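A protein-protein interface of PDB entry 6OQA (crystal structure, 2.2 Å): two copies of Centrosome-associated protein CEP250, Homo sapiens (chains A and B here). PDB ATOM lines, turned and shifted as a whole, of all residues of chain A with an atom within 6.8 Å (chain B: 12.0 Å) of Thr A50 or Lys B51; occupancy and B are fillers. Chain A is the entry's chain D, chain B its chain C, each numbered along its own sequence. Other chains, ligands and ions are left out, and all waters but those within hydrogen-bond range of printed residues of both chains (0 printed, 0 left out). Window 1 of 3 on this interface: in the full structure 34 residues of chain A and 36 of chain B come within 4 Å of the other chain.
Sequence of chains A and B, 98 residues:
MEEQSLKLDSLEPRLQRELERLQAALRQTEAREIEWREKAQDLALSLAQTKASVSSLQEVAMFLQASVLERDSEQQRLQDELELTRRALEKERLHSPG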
ATOM      1  N   LEU A  45       0.789  11.055 -19.376  1.00  0.00           N
ATOM      2  CA  LEU A  45      -0.642  11.309 -19.598  1.00  0.00           C
ATOM      3  C   LEU A  45      -1.351  11.784 -18.322  1.00  0.00           C
ATOM      4  O   LEU A  45      -2.197  12.670 -18.388  1.00  0.00           O
ATOM      5  CB  LEU A  45      -1.340  10.057 -20.149  1.00  0.00           C
ATOM      6  CG  LEU A  45      -2.708  10.287 -20.804  1.00  0.00           C
ATOM      7  CD1 LEU A  45      -2.554  11.017 -22.131  1.00  0.00           C
ATOM      8  CD2 LEU A  45      -3.448   8.973 -21.008  1.00  0.00           C
ATOM      9  N   SER A  46      -1.014  11.196 -17.171  1.00  0.00           N
ATOM     10  CA  SER A  46      -1.566  11.650 -15.885  1.00  0.00           C
ATOM     11  C   SER A  46      -1.185  13.094 -15.598  1.00  0.00           C
ATOM     12  O   SER A  46      -2.029  13.886 -15.167  1.00  0.00           O
ATOM     13  CB  SER A  46      -1.094  10.771 -14.723  1.00  0.00           C
ATOM     14  OG  SER A  46      -1.622   9.468 -14.830  1.00  0.00           O
ATOM     15  N   LEU A  47       0.083  13.424 -15.843  1.00  0.00           N
ATOM     16  CA  LEU A  47       0.595  14.775 -15.624  1.00  0.00           C
ATOM     17  C   LEU A  47      -0.100  15.805 -16.505  1.00  0.00           C
ATOM     18  O   LEU A  47      -0.461  16.881 -16.030  1.00  0.00           O
ATOM     19  CB  LEU A  47       2.107  14.838 -15.883  1.00  0.00           C
ATOM     20  CG  LEU A  47       2.828  16.162 -15.599  1.00  0.00           C
ATOM     21  CD1 LEU A  47       2.562  16.663 -14.187  1.00  0.00           C
ATOM     22  CD2 LEU A  47       4.329  15.991 -15.827  1.00  0.00           C
ATOM     23  N   ALA A  48      -0.247  15.494 -17.791  1.00  0.00           N
ATOM     24  CA  ALA A  48      -0.904  16.413 -18.734  1.00  0.00           C
ATOM     25  C   ALA A  48      -2.356  16.663 -18.302  1.00  0.00           C
ATOM     26  O   ALA A  48      -2.821  17.798 -18.322  1.00  0.00           O
ATOM     27  CB  ALA A  48      -0.844  15.874 -20.163  1.00  0.00           C
ATOM     28  N   GLN A  49      -3.045  15.601 -17.884  1.00  0.00           N
ATOM     29  CA  GLN A  49      -4.412  15.725 -17.372  1.00  0.00           C
ATOM     30  C   GLN A  49      -4.463  16.481 -16.047  1.00  0.00           C
ATOM     31  O   GLN A  49      -5.392  17.263 -15.827  1.00  0.00           O
ATOM     32  CB  GLN A  49      -5.088  14.356 -17.244  1.00  0.00           C
ATOM     33  CG  GLN A  49      -5.598  13.809 -18.570  1.00  0.00           C
ATOM     34  CD  GLN A  49      -6.914  14.439 -19.009  1.00  0.00           C
ATOM     35  OE1 GLN A  49      -6.967  15.174 -19.993  1.00  0.00           O
ATOM     36  NE2 GLN A  49      -7.978  14.159 -18.269  1.00  0.00           N
ATOM     37  N   THR A  50      -3.471  16.263 -15.175  1.00  0.00           N
ATOM     38  CA  THR A  50      -3.393  17.002 -13.901  1.00  0.00           C
ATOM     39  C   THR A  50      -3.044  18.485 -14.146  1.00  0.00           C
ATOM     40  O   THR A  50      -3.616  19.362 -13.513  1.00  0.00           O
ATOM     41  CB  THR A  50      -2.406  16.356 -12.884  1.00  0.00           C
ATOM     42  OG1 THR A  50      -2.632  14.945 -12.819  1.00  0.00           O
ATOM     43  CG2 THR A  50      -2.625  16.920 -11.504  1.00  0.00           C
ATOM     44  N   LYS A  51      -2.130  18.764 -15.068  1.00  0.00           N
ATOM     45  CA  LYS A  51      -1.855  20.151 -15.502  1.00  0.00           C
ATOM     46  C   LYS A  51      -3.101  20.835 -16.093  1.00  0.00           C
ATOM     47  O   LYS A  51      -3.355  22.015 -15.826  1.00  0.00           O
ATOM     48  CB  LYS A  51      -0.718  20.205 -16.530  1.00  0.00           C
ATOM     49  CG  LYS A  51       0.681  20.029 -15.941  1.00  0.00           C
ATOM     50  CD  LYS A  51       1.732  19.961 -17.046  1.00  0.00           C
ATOM     51  CE  LYS A  51       3.140  20.185 -16.515  1.00  0.00           C
ATOM     52  N   ALA A  52      -3.869  20.097 -16.895  1.00  0.00           N
ATOM     53  CA  ALA A  52      -5.134  20.625 -17.448  1.00  0.00           C
ATOM     54  C   ALA A  52      -6.096  21.003 -16.314  1.00  0.00           C
ATOM     55  O   ALA A  52      -6.691  22.077 -16.326  1.00  0.00           O
ATOM     56  CB  ALA A  52      -5.776  19.606 -18.379  1.00  0.00           C
ATOM     57  N   SER A  53      -6.201  20.113 -15.329  1.00  0.00           N
ATOM     58  CA  SER A  53      -6.983  20.334 -14.106  1.00  0.00           C
ATOM     59  C   SER A  53      -6.615  21.620 -13.362  1.00  0.00           C
ATOM     60  O   SER A  53      -7.505  22.328 -12.900  1.00  0.00           O
ATOM     61  CB  SER A  53      -6.845  19.130 -13.159  1.00  0.00           C
ATOM     62  OG  SER A  53      -7.805  19.183 -12.129  1.00  0.00           O
ATOM     63  N   VAL A  54      -5.317  21.915 -13.250  1.00  0.00           N
ATOM     64  CA  VAL A  54      -4.831  23.171 -12.641  1.00  0.00           C
ATOM     65  C   VAL A  54      -5.322  24.396 -13.410  1.00  0.00           C
ATOM     66  O   VAL A  54      -5.811  25.354 -12.808  1.00  0.00           O
ATOM     67  CB  VAL A  54      -3.271  23.227 -12.562  1.00  0.00           C
ATOM     68  CG1 VAL A  54      -2.780  24.628 -12.207  1.00  0.00           C
ATOM     69  CG2 VAL A  54      -2.745  22.218 -11.557  1.00  0.00           C
ATOM     70  N   SER A  55      -5.154  24.377 -14.735  1.00  0.00           N
ATOM     71  CA  SER A  55      -5.647  25.460 -15.590  1.00  0.00           C
ATOM     72  C   SER A  55      -7.149  25.664 -15.428  1.00  0.00           C
ATOM     73  O   SER A  55      -7.603  26.797 -15.299  1.00  0.00           O
ATOM     74  CB  SER A  55      -5.331  25.198 -17.069  1.00  0.00           C
ATOM     75  OG  SER A  55      -3.943  25.292 -17.301  1.00  0.00           O
ATOM     76  N   ASP B  42      11.162  11.347 -12.598  1.00  0.00           N
ATOM     77  CA  ASP B  42      10.936  12.795 -12.638  1.00  0.00           C
ATOM     78  C   ASP B  42       9.467  13.182 -12.907  1.00  0.00           C
ATOM     79  O   ASP B  42       8.956  14.139 -12.313  1.00  0.00           O
ATOM     80  CB  ASP B  42      11.854  13.451 -13.667  1.00  0.00           C
ATOM     81  CG  ASP B  42      13.341  13.313 -13.315  1.00  0.00           C
ATOM     82  OD1 ASP B  42      13.670  12.797 -12.221  1.00  0.00           O
ATOM     83  OD2 ASP B  42      14.181  13.712 -14.150  1.00  0.00           O
ATOM     84  N   LEU B  43       8.797  12.440 -13.789  1.00  0.00           N
ATOM     85  CA  LEU B  43       7.356  12.649 -14.038  1.00  0.00           C
ATOM     86  C   LEU B  43       6.508  12.310 -12.811  1.00  0.00           C
ATOM     87  O   LEU B  43       5.521  12.992 -12.543  1.00  0.00           O
ATOM     88  CB  LEU B  43       6.880  11.847 -15.257  1.00  0.00           C
ATOM     89  CG  LEU B  43       7.421  12.331 -16.612  1.00  0.00           C
ATOM     90  CD1 LEU B  43       7.110  11.315 -17.703  1.00  0.00           C
ATOM     91  CD2 LEU B  43       6.888  13.710 -16.993  1.00  0.00           C
ATOM     92  N   ALA B  44       6.901  11.277 -12.061  1.00  0.00           N
ATOM     93  CA  ALA B  44       6.199  10.903 -10.821  1.00  0.00           C
ATOM     94  C   ALA B  44       6.310  11.989  -9.751  1.00  0.00           C
ATOM     95  O   ALA B  44       5.338  12.288  -9.041  1.00  0.00           O
ATOM     96  CB  ALA B  44       6.730   9.580 -10.279  1.00  0.00           C
ATOM     97  N   LEU B  45       7.503  12.565  -9.633  1.00  0.00           N
ATOM     98  CA  LEU B  45       7.737  13.667  -8.714  1.00  0.00           C
ATOM     99  C   LEU B  45       6.959  14.912  -9.150  1.00  0.00           C
ATOM    100  O   LEU B  45       6.324  15.564  -8.330  1.00  0.00           O
ATOM    101  CB  LEU B  45       9.236  13.975  -8.618  1.00  0.00           C
ATOM    102  CG  LEU B  45       9.652  15.067  -7.625  1.00  0.00           C
ATOM    103  CD1 LEU B  45       9.160  14.726  -6.231  1.00  0.00           C
ATOM    104  CD2 LEU B  45      11.162  15.243  -7.629  1.00  0.00           C
ATOM    105  N   SER B  46       7.010  15.229 -10.438  1.00  0.00           N
ATOM    106  CA  SER B  46       6.290  16.378 -10.968  1.00  0.00           C
ATOM    107  C   SER B  46       4.772  16.204 -10.795  1.00  0.00           C
ATOM    108  O   SER B  46       4.078  17.163 -10.449  1.00  0.00           O
ATOM    109  CB  SER B  46       6.654  16.613 -12.434  1.00  0.00           C
ATOM    110  OG  SER B  46       5.887  17.670 -12.980  1.00  0.00           O
ATOM    111  N   LEU B  47       4.279  14.980 -11.005  1.00  0.00           N
ATOM    112  CA  LEU B  47       2.854  14.656 -10.806  1.00  0.00           C
ATOM    113  C   LEU B  47       2.419  14.897  -9.357  1.00  0.00           C
ATOM    114  O   LEU B  47       1.398  15.546  -9.123  1.00  0.00           O
ATOM    115  CB  LEU B  47       2.552  13.208 -11.220  1.00  0.00           C
ATOM    116  CG  LEU B  47       1.102  12.708 -11.139  1.00  0.00           C
ATOM    117  CD1 LEU B  47       0.162  13.527 -12.025  1.00  0.00           C
ATOM    118  CD2 LEU B  47       1.047  11.236 -11.517  1.00  0.00           C
ATOM    119  N   ALA B  48       3.205  14.409  -8.392  1.00  0.00           N
ATOM    120  CA  ALA B  48       2.889  14.601  -6.964  1.00  0.00           C
ATOM    121  C   ALA B  48       2.797  16.087  -6.592  1.00  0.00           C
ATOM    122  O   ALA B  48       1.884  16.491  -5.878  1.00  0.00           O
ATOM    123  CB  ALA B  48       3.910  13.887  -6.074  1.00  0.00           C
ATOM    124  N   GLN B  49       3.734  16.883  -7.106  1.00  0.00           N
ATOM    125  CA  GLN B  49       3.765  18.337  -6.888  1.00  0.00           C
ATOM    126  C   GLN B  49       2.585  19.089  -7.540  1.00  0.00           C
ATOM    127  O   GLN B  49       2.009  19.991  -6.927  1.00  0.00           O
ATOM    128  CB  GLN B  49       5.096  18.923  -7.387  1.00  0.00           C
ATOM    129  CG  GLN B  49       6.311  18.436  -6.597  1.00  0.00           C
ATOM    130  CD  GLN B  49       7.651  18.826  -7.202  1.00  0.00           C
ATOM    131  OE1 GLN B  49       7.789  18.969  -8.416  1.00  0.00           O
ATOM    132  NE2 GLN B  49       8.657  18.968  -6.347  1.00  0.00           N
ATOM    133  N   THR B  50       2.244  18.723  -8.773  1.00  0.00           N
ATOM    134  CA  THR B  50       1.081  19.296  -9.466  1.00  0.00           C
ATOM    135  C   THR B  50      -0.234  18.926  -8.771  1.00  0.00           C
ATOM    136  O   THR B  50      -1.148  19.745  -8.700  1.00  0.00           O
ATOM    137  CB  THR B  50       1.004  18.844 -10.939  1.00  0.00           C
ATOM    138  OG1 THR B  50       2.306  18.894 -11.524  1.00  0.00           O
ATOM    139  CG2 THR B  50       0.064  19.745 -11.728  1.00  0.00           C
ATOM    140  N   LYS B  51      -0.314  17.693  -8.263  1.00  0.00           N
ATOM    141  CA  LYS B  51      -1.455  17.247  -7.455  1.00  0.00           C
ATOM    142  C   LYS B  51      -1.651  18.076  -6.182  1.00  0.00           C
ATOM    143  O   LYS B  51      -2.789  18.313  -5.779  1.00  0.00           O
ATOM    144  CB  LYS B  51      -1.344  15.756  -7.113  1.00  0.00           C
ATOM    145  CG  LYS B  51      -1.765  14.833  -8.257  1.00  0.00           C
ATOM    146  CD  LYS B  51      -1.893  13.388  -7.796  1.00  0.00           C
ATOM    147  CE  LYS B  51      -2.739  12.565  -8.757  1.00  0.00           C
ATOM    148  N   ALA B  52      -0.553  18.529  -5.567  1.00  0.00           N
ATOM    149  CA  ALA B  52      -0.633  19.440  -4.417  1.00  0.00           C
ATOM    150  C   ALA B  52      -1.173  20.820  -4.826  1.00  0.00           C
ATOM    151  O   ALA B  52      -1.991  21.398  -4.106  1.00  0.00           O
ATOM    152  CB  ALA B  52       0.719  19.580  -3.733  1.00  0.00           C
ATOM    153  N   SER B  53      -0.727  21.340  -5.971  1.00  0.00           N
ATOM    154  CA  SER B  53      -1.248  22.623  -6.475  1.00  0.00           C
ATOM    155  C   SER B  53      -2.745  22.533  -6.852  1.00  0.00           C
ATOM    156  O   SER B  53      -3.482  23.506  -6.681  1.00  0.00           O
ATOM    157  CB  SER B  53      -0.419  23.145  -7.657  1.00  0.00           C
ATOM    158  OG  SER B  53      -0.628  22.368  -8.817  1.00  0.00           O
ATOM    159  N   VAL B  54      -3.178  21.367  -7.337  1.00  0.00           N
ATOM    160  CA  VAL B  54      -4.608  21.091  -7.582  1.00  0.00           C
ATOM    161  C   VAL B  54      -5.412  21.208  -6.281  1.00  0.00           C
ATOM    162  O   VAL B  54      -6.421  21.910  -6.236  1.00  0.00           O
ATOM    163  CB  VAL B  54      -4.828  19.708  -8.244  1.00  0.00           C
ATOM    164  CG1 VAL B  54      -6.307  19.347  -8.294  1.00  0.00           C
ATOM    165  CG2 VAL B  54      -4.223  19.682  -9.643  1.00  0.00           C
ATOM    166  N   SER B  55      -4.935  20.571  -5.213  1.00  0.00           N
ATOM    167  CA  SER B  55      -5.602  20.665  -3.909  1.00  0.00           C
ATOM    168  C   SER B  55      -5.665  22.092  -3.379  1.00  0.00           C
ATOM    169  O   SER B  55      -6.713  22.534  -2.924  1.00  0.00           O
ATOM    170  CB  SER B  55      -4.937  19.753  -2.871  1.00  0.00           C
ATOM    171  OG  SER B  55      -5.156  18.401  -3.220  1.00  0.00           O
ATOM    172  N   SER B  56      -4.550  22.811  -3.452  1.00  0.00           N
ATOM    173  CA  SER B  56      -4.499  24.200  -3.007  1.00  0.00           C
ATOM    174  C   SER B  56      -5.467  25.133  -3.770  1.00  0.00           C
ATOM    175  O   SER B  56      -6.092  26.012  -3.166  1.00  0.00           O
ATOM    176  CB  SER B  56      -3.062  24.736  -3.125  1.00  0.00           C
ATOM    177  OG  SER B  56      -2.177  24.053  -2.246  1.00  0.00           O
ATOM    178  N   LEU B  57      -5.578  24.955  -5.087  1.00  0.00           N
ATOM    179  CA  LEU B  57      -6.503  25.767  -5.903  1.00  0.00           C
ATOM    180  C   LEU B  57      -7.961  25.433  -5.612  1.00  0.00           C
ATOM    181  O   LEU B  57      -8.802  26.326  -5.606  1.00  0.00           O
ATOM    182  CB  LEU B  57      -6.205  25.632  -7.411  1.00  0.00           C
ATOM    183  CG  LEU B  57      -4.946  26.338  -7.915  1.00  0.00           C
ATOM    184  CD1 LEU B  57      -4.655  25.982  -9.370  1.00  0.00           C
ATOM    185  CD2 LEU B  57      -5.072  27.844  -7.749  1.00  0.00           C
ATOM    186  N   GLN B  58      -8.247  24.153  -5.362  1.00  0.00           N
ATOM    187  CA  GLN B  58      -9.571  23.708  -4.865  1.00  0.00           C
ATOM    188  C   GLN B  58      -9.958  24.452  -3.580  1.00  0.00           C
ATOM    189  O   GLN B  58     -11.104  24.920  -3.430  1.00  0.00           O
ATOM    190  CB  GLN B  58      -9.599  22.165  -4.690  1.00  0.00           C
ATOM    191  CG  GLN B  58     -10.452  21.571  -3.561  1.00  0.00           C
ATOM    192  CD  GLN B  58     -11.885  21.268  -3.957  1.00  0.00           C
ATOM    193  OE1 GLN B  58     -12.820  21.937  -3.513  1.00  0.00           O
ATOM    194  NE2 GLN B  58     -12.066  20.242  -4.777  1.00  0.00           N
ATOM    195  N   GLU B  59      -8.999  24.576  -2.666  1.00  0.00           N
ATOM    196  CA  GLU B  59      -9.241  25.280  -1.405  1.00  0.00           C
ATOM    197  C   GLU B  59      -9.389  26.776  -1.631  1.00  0.00           C
ATOM    198  O   GLU B  59     -10.187  27.400  -0.952  1.00  0.00           O
ATOM    199  CB  GLU B  59      -8.137  24.986  -0.378  1.00  0.00           C
ATOM    200  CG  GLU B  59      -8.137  23.538   0.086  1.00  0.00           C
ATOM    201  CD  GLU B  59      -7.353  23.313   1.369  1.00  0.00           C
ATOM    202  OE1 GLU B  59      -6.396  24.072   1.646  1.00  0.00           O
ATOM    203  OE2 GLU B  59      -7.697  22.364   2.099  1.00  0.00           O
ATOM    204  N   VAL B  60      -8.634  27.346  -2.582  1.00  0.00           N
ATOM    205  CA  VAL B  60      -8.822  28.761  -2.968  1.00  0.00           C
ATOM    206  C   VAL B  60     -10.246  28.977  -3.535  1.00  0.00           C
ATOM    207  O   VAL B  60     -10.957  29.895  -3.110  1.00  0.00           O
ATOM    208  CB  VAL B  60      -7.716  29.258  -3.933  1.00  0.00           C
ATOM    209  CG1 VAL B  60      -8.011  30.665  -4.449  1.00  0.00           C
ATOM    210  CG2 VAL B  60      -6.349  29.236  -3.239  1.00  0.00           C
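Thr A50 touches just these residues of chain B: Leu B47, Thr B50, Lys B51 and Val B54. Lys B51 touches just one residue of chain A: Thr A50. Leu A47 touches just these residues of chain B: Leu B43, Ser B46, Leu B47 and Thr B50. No residue of chain B comes within 4 Å of Ala A48. Of the printed residues of chain A, Leu B43 touches Leu A47. Of the printed residues of chain A, Leu B47 touches Ser A46 (3.8 Å), Leu A47 (3.8 Å) and Thr A50 (3.2 Å). Of the printed residues of chain A, Leu B57 touches Val A54. Of the printed residues of chain A, Thr B50 touches Leu A47 (3.5 Å), Thr A50 (3.9 Å) and Val A54 (3.7 Å). Of the printed residues of chain A, Ser B53 touches Val A54. Ala B48 touches none of the printed residues of chain A.
Among the printed residues, merely in contact across the chains: Thr A50 with Leu B47 (3.2 Å), Val A54 with Ser B53 (3.5 Å), Leu A47 with Thr B50 (3.5 Å), Val A54 with Val B54 (3.5 Å), Leu A47 with Leu B43 (3.6 Å), Leu A47 with Ser B46 (3.7 Å), Val A54 with Leu B57 (3.7 Å), Thr A50 with Val B54 (3.7 Å), Val A54 with Thr B50 (3.7 Å), Leu A47 with Leu B47 (3.8 Å), Ser A46 with Leu B47 (3.8 Å), Thr A50 with Thr B50 (3.9 Å) and Thr A50 with Lys B51 (3.95 Å).
Printed residues of chain A that touch a printed residue of chain B: Ser A46, Leu A47, Thr A50 and Val A54. Among the printed residues, no Asp or Glu carboxylate lies within 4 Å of a Lys or Arg side-chain nitrogen of the other chain.
Leu B47 touches its own counterpart, Leu A47. Leu A47 touches Thr B50, and with the chains exchanged Thr A50 touches Leu B47. Thr A50 touches Lys B51, but with the chains exchanged Lys A51 does not touch Thr B50 (4.1 Å). Thr A50 touches Val B54, and with the chains exchanged Val A54 touches Thr B50. 11 positions are printed for both chains. Of the 13 pairs that touch across the chains among the printed residues, 9 have their exchanged pair printed and touching as well.
The side-chain hydroxyl (OG1) of Thr B50 is in hydrogen-bond range of the backbone carbonyl oxygen (O) of Ser B46 (2.7 Å). The backbone carbonyl oxygen (O) of Thr B50 is in hydrogen-bond range of the side-chain hydroxyl (OG) of Ser B53, 2.7 Å away. O of Lys B51 lies within hydrogen-bond range of OG of Ser B55 (3.5 Å). O of Ser A46 is in hydrogen-bond range of OG1 of Thr A50, at 2.6 Å.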
